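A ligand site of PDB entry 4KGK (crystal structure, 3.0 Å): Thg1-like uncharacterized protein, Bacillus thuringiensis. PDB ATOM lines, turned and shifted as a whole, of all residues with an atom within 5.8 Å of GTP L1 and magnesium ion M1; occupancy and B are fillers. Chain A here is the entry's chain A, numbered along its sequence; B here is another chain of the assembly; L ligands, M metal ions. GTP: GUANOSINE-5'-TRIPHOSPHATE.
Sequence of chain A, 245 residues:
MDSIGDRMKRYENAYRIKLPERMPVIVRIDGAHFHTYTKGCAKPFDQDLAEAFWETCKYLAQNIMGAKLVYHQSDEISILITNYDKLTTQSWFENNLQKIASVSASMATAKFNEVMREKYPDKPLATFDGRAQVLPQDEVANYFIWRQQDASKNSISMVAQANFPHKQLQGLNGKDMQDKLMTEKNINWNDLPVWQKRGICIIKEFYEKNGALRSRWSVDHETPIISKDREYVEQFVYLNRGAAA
Magnesium ion M1 is bound by O3G of GTP L1 (2.4 Å) and O3A of GTP L1 (2.5 Å).
Slightly farther from magnesium ion M1 lies an oxygen (O2A) of GTP L1 (2.7 Å).
The backbone carbonyl oxygen (O) of Arg 131 of chain B lies within hydrogen-bond range of the backbone NH (N) of Arg 28 of chain B.
The side-chain carboxylate (OD2) of Asp 6 sits at hydrogen-bond distance from the side-chain hydroxyl (OG) of Ser 3 (2.7 Å).
ND2 of Asn 13 is in hydrogen-bond range of O of Lys 9, at 3.0 Å.
The side-chain carboxylate of Glu 12 lies within salt-bridge range of the guanidinium group of Arg 28 of chain B, 3.1 Å away.
NH2 of Arg 131 of chain B is in salt-bridge range of OD2 of Asp 129 of chain B.
OE2 of Glu 12 is in salt-bridge range of NH1 of Arg 131 of chain B (3.0 Å).
No residue comes within 4 Å of magnesium ion M1.
The guanidinium group (NH1) of Arg 16 is in salt-bridge range of an oxygen (O2G) of GTP L1, 3.4 Å away.
The guanidinium group (NH2) of Arg 28 of chain B lies within salt-bridge range of an oxygen (O1A) of GTP L1 (3.6 Å).
NH1 of Arg 131 of chain B lies within salt-bridge range of O2G of GTP L1 (2.8 Å).
N2 of GTP L1 lies close to O of Gly 5 (3.4 Å).
Asp 6 touches GTP L1.
CB of Lys 9 touches O6 of GTP L1, 3.8 Å away.
Lys 99 touches GTP L1 (CE to O3G, 3.5 Å).
Trp 146 of chain B touches GTP L1.
Hydrophobic or aromatic side chains within 4 Å of GTP L1: Trp 146 of chain B.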
ATOM      1  N   SER A   3     -17.038   1.800   4.905  1.00  0.00           N
ATOM      2  CA  SER A   3     -17.814   2.421   3.829  1.00  0.00           C
ATOM      3  C   SER A   3     -17.448   1.827   2.475  1.00  0.00           C
ATOM      4  O   SER A   3     -16.625   0.918   2.393  1.00  0.00           O
ATOM      5  CB  SER A   3     -17.603   3.934   3.822  1.00  0.00           C
ATOM      6  OG  SER A   3     -16.238   4.265   3.675  1.00  0.00           O
ATOM      7  N   ILE A   4     -18.060   2.353   1.418  1.00  0.00           N
ATOM      8  CA  ILE A   4     -17.794   1.874   0.067  1.00  0.00           C
ATOM      9  C   ILE A   4     -16.522   2.508  -0.495  1.00  0.00           C
ATOM     10  O   ILE A   4     -15.922   1.993  -1.438  1.00  0.00           O
ATOM     11  CB  ILE A   4     -18.980   2.130  -0.900  1.00  0.00           C
ATOM     12  CG1 ILE A   4     -18.960   3.566  -1.445  1.00  0.00           C
ATOM     13  CG2 ILE A   4     -20.308   1.810  -0.220  1.00  0.00           C
ATOM     14  CD1 ILE A   4     -19.329   4.634  -0.439  1.00  0.00           C
ATOM     15  N   GLY A   5     -16.121   3.637   0.088  1.00  0.00           N
ATOM     16  CA  GLY A   5     -14.913   4.321  -0.329  1.00  0.00           C
ATOM     17  C   GLY A   5     -13.673   3.597   0.139  1.00  0.00           C
ATOM     18  O   GLY A   5     -12.651   3.566  -0.561  1.00  0.00           O
ATOM     19  N   ASP A   6     -13.755   3.009   1.330  1.00  0.00           N
ATOM     20  CA  ASP A   6     -12.638   2.258   1.897  1.00  0.00           C
ATOM     21  C   ASP A   6     -12.412   0.988   1.101  1.00  0.00           C
ATOM     22  O   ASP A   6     -11.271   0.609   0.812  1.00  0.00           O
ATOM     23  CB  ASP A   6     -12.945   1.902   3.355  1.00  0.00           C
ATOM     24  CG  ASP A   6     -13.376   3.096   4.175  1.00  0.00           C
ATOM     25  OD1 ASP A   6     -12.796   4.187   3.996  1.00  0.00           O
ATOM     26  OD2 ASP A   6     -14.309   2.945   5.001  1.00  0.00           O
ATOM     27  N   LYS A   9     -10.880   1.799  -2.487  1.00  0.00           N
ATOM     28  CA  LYS A   9      -9.472   2.161  -2.465  1.00  0.00           C
ATOM     29  C   LYS A   9      -8.621   0.910  -2.232  1.00  0.00           C
ATOM     30  O   LYS A   9      -7.458   0.867  -2.622  1.00  0.00           O
ATOM     31  CB  LYS A   9      -9.198   3.196  -1.386  1.00  0.00           C
ATOM     32  N   GLU A  12      -7.846  -0.683  -5.458  1.00  0.00           N
ATOM     33  CA  GLU A  12      -6.849   0.158  -6.102  1.00  0.00           C
ATOM     34  C   GLU A  12      -5.460  -0.101  -5.541  1.00  0.00           C
ATOM     35  O   GLU A  12      -4.482  -0.226  -6.287  1.00  0.00           O
ATOM     36  CB  GLU A  12      -7.216   1.634  -5.950  1.00  0.00           C
ATOM     37  CG  GLU A  12      -6.223   2.590  -6.587  1.00  0.00           C
ATOM     38  CD  GLU A  12      -6.646   4.031  -6.469  1.00  0.00           C
ATOM     39  OE1 GLU A  12      -7.861   4.286  -6.305  1.00  0.00           O
ATOM     40  OE2 GLU A  12      -5.771   4.916  -6.528  1.00  0.00           O
ATOM     41  N   ASN A  13      -5.366  -0.177  -4.217  1.00  0.00           N
ATOM     42  CA  ASN A  13      -4.096  -0.389  -3.536  1.00  0.00           C
ATOM     43  C   ASN A  13      -3.426  -1.700  -3.919  1.00  0.00           C
ATOM     44  O   ASN A  13      -2.217  -1.865  -3.721  1.00  0.00           O
ATOM     45  CB  ASN A  13      -4.267  -0.310  -2.018  1.00  0.00           C
ATOM     46  CG  ASN A  13      -4.563   1.092  -1.525  1.00  0.00           C
ATOM     47  OD1 ASN A  13      -4.064   2.064  -2.074  1.00  0.00           O
ATOM     48  ND2 ASN A  13      -5.379   1.194  -0.488  1.00  0.00           N
ATOM     49  N   ARG A  16      -0.910  -0.678  -6.283  1.00  0.00           N
ATOM     50  CA  ARG A  16      -0.167   0.523  -5.933  1.00  0.00           C
ATOM     51  C   ARG A  16       1.240   0.106  -5.546  1.00  0.00           C
ATOM     52  O   ARG A  16       1.618   0.122  -4.369  1.00  0.00           O
ATOM     53  CB  ARG A  16      -0.840   1.267  -4.780  1.00  0.00           C
ATOM     54  CG  ARG A  16      -0.272   2.660  -4.534  1.00  0.00           C
ATOM     55  CD  ARG A  16      -0.824   3.254  -3.249  1.00  0.00           C
ATOM     56  NE  ARG A  16      -0.320   4.608  -3.040  1.00  0.00           N
ATOM     57  CZ  ARG A  16      -0.947   5.715  -3.422  1.00  0.00           C
ATOM     58  NH1 ARG A  16      -2.110   5.625  -4.055  1.00  0.00           N
ATOM     59  NH2 ARG A  16      -0.421   6.903  -3.196  1.00  0.00           N
ATOM     60  N   ASN A  96       6.223   5.723  -6.323  1.00  0.00           N
ATOM     61  CA  ASN A  96       5.032   5.085  -6.880  1.00  0.00           C
ATOM     62  C   ASN A  96       5.275   4.689  -8.333  1.00  0.00           C
ATOM     63  O   ASN A  96       5.422   5.548  -9.204  1.00  0.00           O
ATOM     64  CB  ASN A  96       3.835   6.041  -6.767  1.00  0.00           C
ATOM     65  CG  ASN A  96       2.508   5.339  -6.961  1.00  0.00           C
ATOM     66  OD1 ASN A  96       2.395   4.387  -7.743  1.00  0.00           O
ATOM     67  ND2 ASN A  96       1.477   5.806  -6.259  1.00  0.00           N
ATOM     68  N   LYS A  99       2.674   5.868 -11.029  1.00  0.00           N
ATOM     69  CA  LYS A  99       2.661   7.322 -11.098  1.00  0.00           C
ATOM     70  C   LYS A  99       3.914   7.863 -11.785  1.00  0.00           C
ATOM     71  O   LYS A  99       3.842   8.794 -12.588  1.00  0.00           O
ATOM     72  CB  LYS A  99       2.495   7.938  -9.708  1.00  0.00           C
ATOM     73  CG  LYS A  99       1.805   9.297  -9.733  1.00  0.00           C
ATOM     74  CD  LYS A  99       1.200   9.626  -8.381  1.00  0.00           C
ATOM     75  CE  LYS A  99       0.046  10.617  -8.525  1.00  0.00           C
ATOM     76  NZ  LYS A  99       0.450  11.834  -9.270  1.00  0.00           N
ATOM     77  N   ARG B  28      -8.050   4.976 -14.361  1.00  0.00           N
ATOM     78  CA  ARG B  28      -8.379   6.358 -14.010  1.00  0.00           C
ATOM     79  C   ARG B  28      -7.231   7.317 -14.330  1.00  0.00           C
ATOM     80  O   ARG B  28      -6.066   7.025 -14.048  1.00  0.00           O
ATOM     81  CB  ARG B  28      -8.777   6.482 -12.539  1.00  0.00           C
ATOM     82  CG  ARG B  28      -9.372   7.836 -12.190  1.00  0.00           C
ATOM     83  CD  ARG B  28     -10.007   7.859 -10.806  1.00  0.00           C
ATOM     84  NE  ARG B  28      -9.011   7.842  -9.743  1.00  0.00           N
ATOM     85  CZ  ARG B  28      -8.702   6.761  -9.022  1.00  0.00           C
ATOM     86  NH1 ARG B  28      -9.314   5.608  -9.251  1.00  0.00           N
ATOM     87  NH2 ARG B  28      -7.785   6.842  -8.072  1.00  0.00           N
ATOM     88  N   ASP B  30      -6.188  11.170 -13.621  1.00  0.00           N
ATOM     89  CA  ASP B  30      -6.409  12.440 -12.941  1.00  0.00           C
ATOM     90  C   ASP B  30      -5.416  13.477 -13.419  1.00  0.00           C
ATOM     91  O   ASP B  30      -4.292  13.152 -13.806  1.00  0.00           O
ATOM     92  CB  ASP B  30      -6.292  12.255 -11.425  1.00  0.00           C
ATOM     93  CG  ASP B  30      -6.950  13.378 -10.651  1.00  0.00           C
ATOM     94  OD1 ASP B  30      -8.069  13.168 -10.133  1.00  0.00           O
ATOM     95  OD2 ASP B  30      -6.352  14.473 -10.558  1.00  0.00           O
ATOM     96  N   GLY B  31      -5.832  14.743 -13.397  1.00  0.00           N
ATOM     97  CA  GLY B  31      -4.971  15.833 -13.822  1.00  0.00           C
ATOM     98  C   GLY B  31      -3.833  16.087 -12.866  1.00  0.00           C
ATOM     99  O   GLY B  31      -3.932  15.803 -11.666  1.00  0.00           O
ATOM    100  N   ASP B 129      -1.661  11.868 -14.736  1.00  0.00           N
ATOM    101  CA  ASP B 129      -1.194  10.610 -14.169  1.00  0.00           C
ATOM    102  C   ASP B 129      -2.224   9.540 -14.496  1.00  0.00           C
ATOM    103  O   ASP B 129      -3.409   9.836 -14.654  1.00  0.00           O
ATOM    104  CB  ASP B 129      -1.037  10.728 -12.651  1.00  0.00           C
ATOM    105  CG  ASP B 129      -2.356  10.768 -11.920  1.00  0.00           C
ATOM    106  OD1 ASP B 129      -2.885  11.885 -11.688  1.00  0.00           O
ATOM    107  OD2 ASP B 129      -2.879   9.690 -11.563  1.00  0.00           O
ATOM    108  N   ARG B 131      -3.527   5.364 -13.587  1.00  0.00           N
ATOM    109  CA  ARG B 131      -3.434   4.134 -12.812  1.00  0.00           C
ATOM    110  C   ARG B 131      -4.452   3.102 -13.275  1.00  0.00           C
ATOM    111  O   ARG B 131      -5.550   3.452 -13.705  1.00  0.00           O
ATOM    112  CB  ARG B 131      -3.594   4.423 -11.312  1.00  0.00           C
ATOM    113  CG  ARG B 131      -4.995   4.828 -10.892  1.00  0.00           C
ATOM    114  CD  ARG B 131      -4.957   5.606  -9.599  1.00  0.00           C
ATOM    115  NE  ARG B 131      -4.215   6.856  -9.748  1.00  0.00           N
ATOM    116  CZ  ARG B 131      -3.904   7.670  -8.747  1.00  0.00           C
ATOM    117  NH1 ARG B 131      -4.276   7.381  -7.513  1.00  0.00           N
ATOM    118  NH2 ARG B 131      -3.231   8.782  -8.992  1.00  0.00           N
ATOM    119  N   TRP B 146     -19.379   5.375  -6.861  1.00  0.00           N
ATOM    120  CA  TRP B 146     -18.472   6.036  -5.935  1.00  0.00           C
ATOM    121  C   TRP B 146     -17.874   7.306  -6.521  1.00  0.00           C
ATOM    122  O   TRP B 146     -17.712   8.299  -5.822  1.00  0.00           O
ATOM    123  CB  TRP B 146     -17.366   5.066  -5.501  1.00  0.00           C
ATOM    124  CG  TRP B 146     -16.220   5.703  -4.775  1.00  0.00           C
ATOM    125  CD1 TRP B 146     -16.286   6.474  -3.660  1.00  0.00           C
ATOM    126  CD2 TRP B 146     -14.836   5.590  -5.115  1.00  0.00           C
ATOM    127  NE1 TRP B 146     -15.026   6.866  -3.286  1.00  0.00           N
ATOM    128  CE2 TRP B 146     -14.117   6.341  -4.162  1.00  0.00           C
ATOM    129  CE3 TRP B 146     -14.126   4.945  -6.137  1.00  0.00           C
ATOM    130  CZ2 TRP B 146     -12.724   6.450  -4.199  1.00  0.00           C
ATOM    131  CZ3 TRP B 146     -12.757   5.055  -6.169  1.00  0.00           C
ATOM    132  CH2 TRP B 146     -12.065   5.805  -5.202  1.00  0.00           C
ATOM    133  N   ARG B 147     -17.554   7.274  -7.808  1.00  0.00           N
ATOM    134  CA  ARG B 147     -17.030   8.459  -8.488  1.00  0.00           C
ATOM    135  C   ARG B 147     -18.137   9.484  -8.674  1.00  0.00           C
ATOM    136  O   ARG B 147     -17.913  10.689  -8.544  1.00  0.00           O
ATOM    137  CB  ARG B 147     -16.433   8.085  -9.843  1.00  0.00           C
ATOM    138  CG  ARG B 147     -15.343   7.011  -9.790  1.00  0.00           C
ATOM    139  CD  ARG B 147     -13.968   7.586  -9.436  1.00  0.00           C
ATOM    140  NE  ARG B 147     -13.842   7.925  -8.019  1.00  0.00           N
ATOM    141  CZ  ARG B 147     -13.625   9.148  -7.556  1.00  0.00           C
ATOM    142  NH1 ARG B 147     -13.503  10.164  -8.393  1.00  0.00           N
ATOM    143  NH2 ARG B 147     -13.521   9.357  -6.252  1.00  0.00           N
ATOM    144  N   ASP B 150     -19.072  11.152  -5.461  1.00  0.00           N
ATOM    145  CA  ASP B 150     -17.994  12.086  -5.188  1.00  0.00           C
ATOM    146  C   ASP B 150     -18.097  13.313  -6.095  1.00  0.00           C
ATOM    147  O   ASP B 150     -17.691  14.414  -5.730  1.00  0.00           O
ATOM    148  CB  ASP B 150     -16.642  11.402  -5.383  1.00  0.00           C
ATOM    149  CG  ASP B 150     -15.463  12.297  -5.051  1.00  0.00           C
ATOM    150  OD1 ASP B 150     -14.417  12.170  -5.705  1.00  0.00           O
ATOM    151  OD2 ASP B 150     -15.592  13.131  -4.128  1.00  0.00           O
HETATM  152  PG  GTP L   1      -2.712   9.879  -5.268  1.00  0.00           P
HETATM  153  O1G GTP L   1      -1.669  10.215  -4.231  1.00  0.00           O
HETATM  154  O2G GTP L   1      -2.398   8.519  -5.852  1.00  0.00           O
HETATM  155  O3G GTP L   1      -2.716  10.915  -6.368  1.00  0.00           O
HETATM  156  O3B GTP L   1      -4.135   9.805  -4.519  1.00  0.00           O
HETATM  157  PB  GTP L   1      -4.908  11.153  -4.057  1.00  0.00           P
HETATM  158  O1B GTP L   1      -3.893  12.281  -3.996  1.00  0.00           O
HETATM  159  O2B GTP L   1      -5.591  10.952  -2.722  1.00  0.00           O
HETATM  160  O3A GTP L   1      -5.943  11.469  -5.267  1.00  0.00           O
HETATM  161  PA  GTP L   1      -6.774  10.307  -6.045  1.00  0.00           P
HETATM  162  O1A GTP L   1      -6.568   8.955  -5.399  1.00  0.00           O
HETATM  163  O2A GTP L   1      -6.388  10.296  -7.512  1.00  0.00           O
HETATM  164  O5' GTP L   1      -8.325  10.708  -5.856  1.00  0.00           O
HETATM  165  C5' GTP L   1      -9.258   9.741  -5.419  1.00  0.00           C
HETATM  166  C4' GTP L   1     -10.142  10.397  -4.375  1.00  0.00           C
HETATM  167  O4' GTP L   1     -10.528   9.467  -3.382  1.00  0.00           O
HETATM  168  C3' GTP L   1      -9.393  11.511  -3.674  1.00  0.00           C
HETATM  169  O3' GTP L   1      -9.878  12.777  -4.063  1.00  0.00           O
HETATM  170  C2' GTP L   1      -9.585  11.298  -2.193  1.00  0.00           C
HETATM  171  O2' GTP L   1     -10.321  12.363  -1.624  1.00  0.00           O
HETATM  172  C1' GTP L   1     -10.354   9.991  -2.076  1.00  0.00           C
HETATM  173  N9  GTP L   1      -9.547   9.017  -1.337  1.00  0.00           N
HETATM  174  C8  GTP L   1      -8.188   8.860  -1.396  1.00  0.00           C
HETATM  175  N7  GTP L   1      -7.825   7.856  -0.578  1.00  0.00           N
HETATM  176  C5  GTP L   1      -8.940   7.351  -0.007  1.00  0.00           C
HETATM  177  C6  GTP L   1      -9.137   6.318   0.903  1.00  0.00           C
HETATM  178  O6  GTP L   1      -8.167   5.679   1.322  1.00  0.00           O
HETATM  179  N1  GTP L   1     -10.406   6.018   1.327  1.00  0.00           N
HETATM  180  C2  GTP L   1     -11.481   6.748   0.850  1.00  0.00           C
HETATM  181  N2  GTP L   1     -12.718   6.461   1.265  1.00  0.00           N
HETATM  182  N3  GTP L   1     -11.287   7.778  -0.050  1.00  0.00           N
HETATM  183  C4  GTP L   1     -10.029   8.073  -0.468  1.00  0.00           C
HETATM  184  PG  GTP L   2      -3.521  16.248  -7.924  1.00  0.00           P
HETATM  185  O1G GTP L   2      -2.358  16.650  -8.807  1.00  0.00           O
HETATM  186  O2G GTP L   2      -3.002  15.455  -6.746  1.00  0.00           O
HETATM  187  O3G GTP L   2      -4.508  15.415  -8.690  1.00  0.00           O
HETATM  188  O3B GTP L   2      -4.221  17.598  -7.390  1.00  0.00           O
HETATM  189  PB  GTP L   2      -4.762  18.696  -8.443  1.00  0.00           P
HETATM  190  O1B GTP L   2      -4.534  18.179  -9.845  1.00  0.00           O
HETATM  191  O2B GTP L   2      -4.089  20.035  -8.236  1.00  0.00           O
HETATM  192  O3A GTP L   2      -6.356  18.810  -8.232  1.00  0.00           O
HETATM  193  PA  GTP L   2      -7.313  17.563  -7.904  1.00  0.00           P
HETATM  194  O1A GTP L   2      -6.913  16.891  -6.609  1.00  0.00           O
HETATM  195  O2A GTP L   2      -7.349  16.592  -9.065  1.00  0.00           O
HETATM  196  O5' GTP L   2      -8.750  18.277  -7.681  1.00  0.00           O
HETATM  197  C5' GTP L   2      -9.423  18.911  -8.748  1.00  0.00           C
HETATM  198  C4' GTP L   2      -8.945  20.359  -8.905  1.00  0.00           C
HETATM  199  O4' GTP L   2      -9.140  20.788 -10.240  1.00  0.00           O
HETATM  200  C3' GTP L   2      -9.690  21.359  -8.025  1.00  0.00           C
HETATM  201  O3' GTP L   2      -8.903  21.700  -6.914  1.00  0.00           O
HETATM  202  C2' GTP L   2      -9.885  22.590  -8.890  1.00  0.00           C
HETATM  203  O2' GTP L   2      -9.017  23.619  -8.467  1.00  0.00           O
HETATM  204  C1' GTP L   2      -9.524  22.153 -10.301  1.00  0.00           C
HETATM  205  N9  GTP L   2     -10.718  22.195 -11.154  1.00  0.00           N
HETATM  206  C8  GTP L   2     -11.320  21.114 -11.735  1.00  0.00           C
HETATM  207  N7  GTP L   2     -12.373  21.527 -12.456  1.00  0.00           N
HETATM  208  C5  GTP L   2     -12.455  22.876 -12.358  1.00  0.00           C
HETATM  209  C6  GTP L   2     -13.341  23.792 -12.909  1.00  0.00           C
HETATM  210  O6  GTP L   2     -14.253  23.396 -13.629  1.00  0.00           O
HETATM  211  N1  GTP L   2     -13.184  25.131 -12.634  1.00  0.00           N
HETATM  212  C2  GTP L   2     -12.144  25.546 -11.822  1.00  0.00           C
HETATM  213  N2  GTP L   2     -11.992  26.843 -11.559  1.00  0.00           N
HETATM  214  N3  GTP L   2     -11.264  24.630 -11.283  1.00  0.00           N
HETATM  215  C4  GTP L   2     -11.410  23.314 -11.549  1.00  0.00           C
HETATM  216 MG    MG M   1      -4.553  12.231  -7.213  1.00  0.00          MG
HETATM  217 MG    MG M   2      -5.678  16.552 -10.748  1.00  0.00          MG
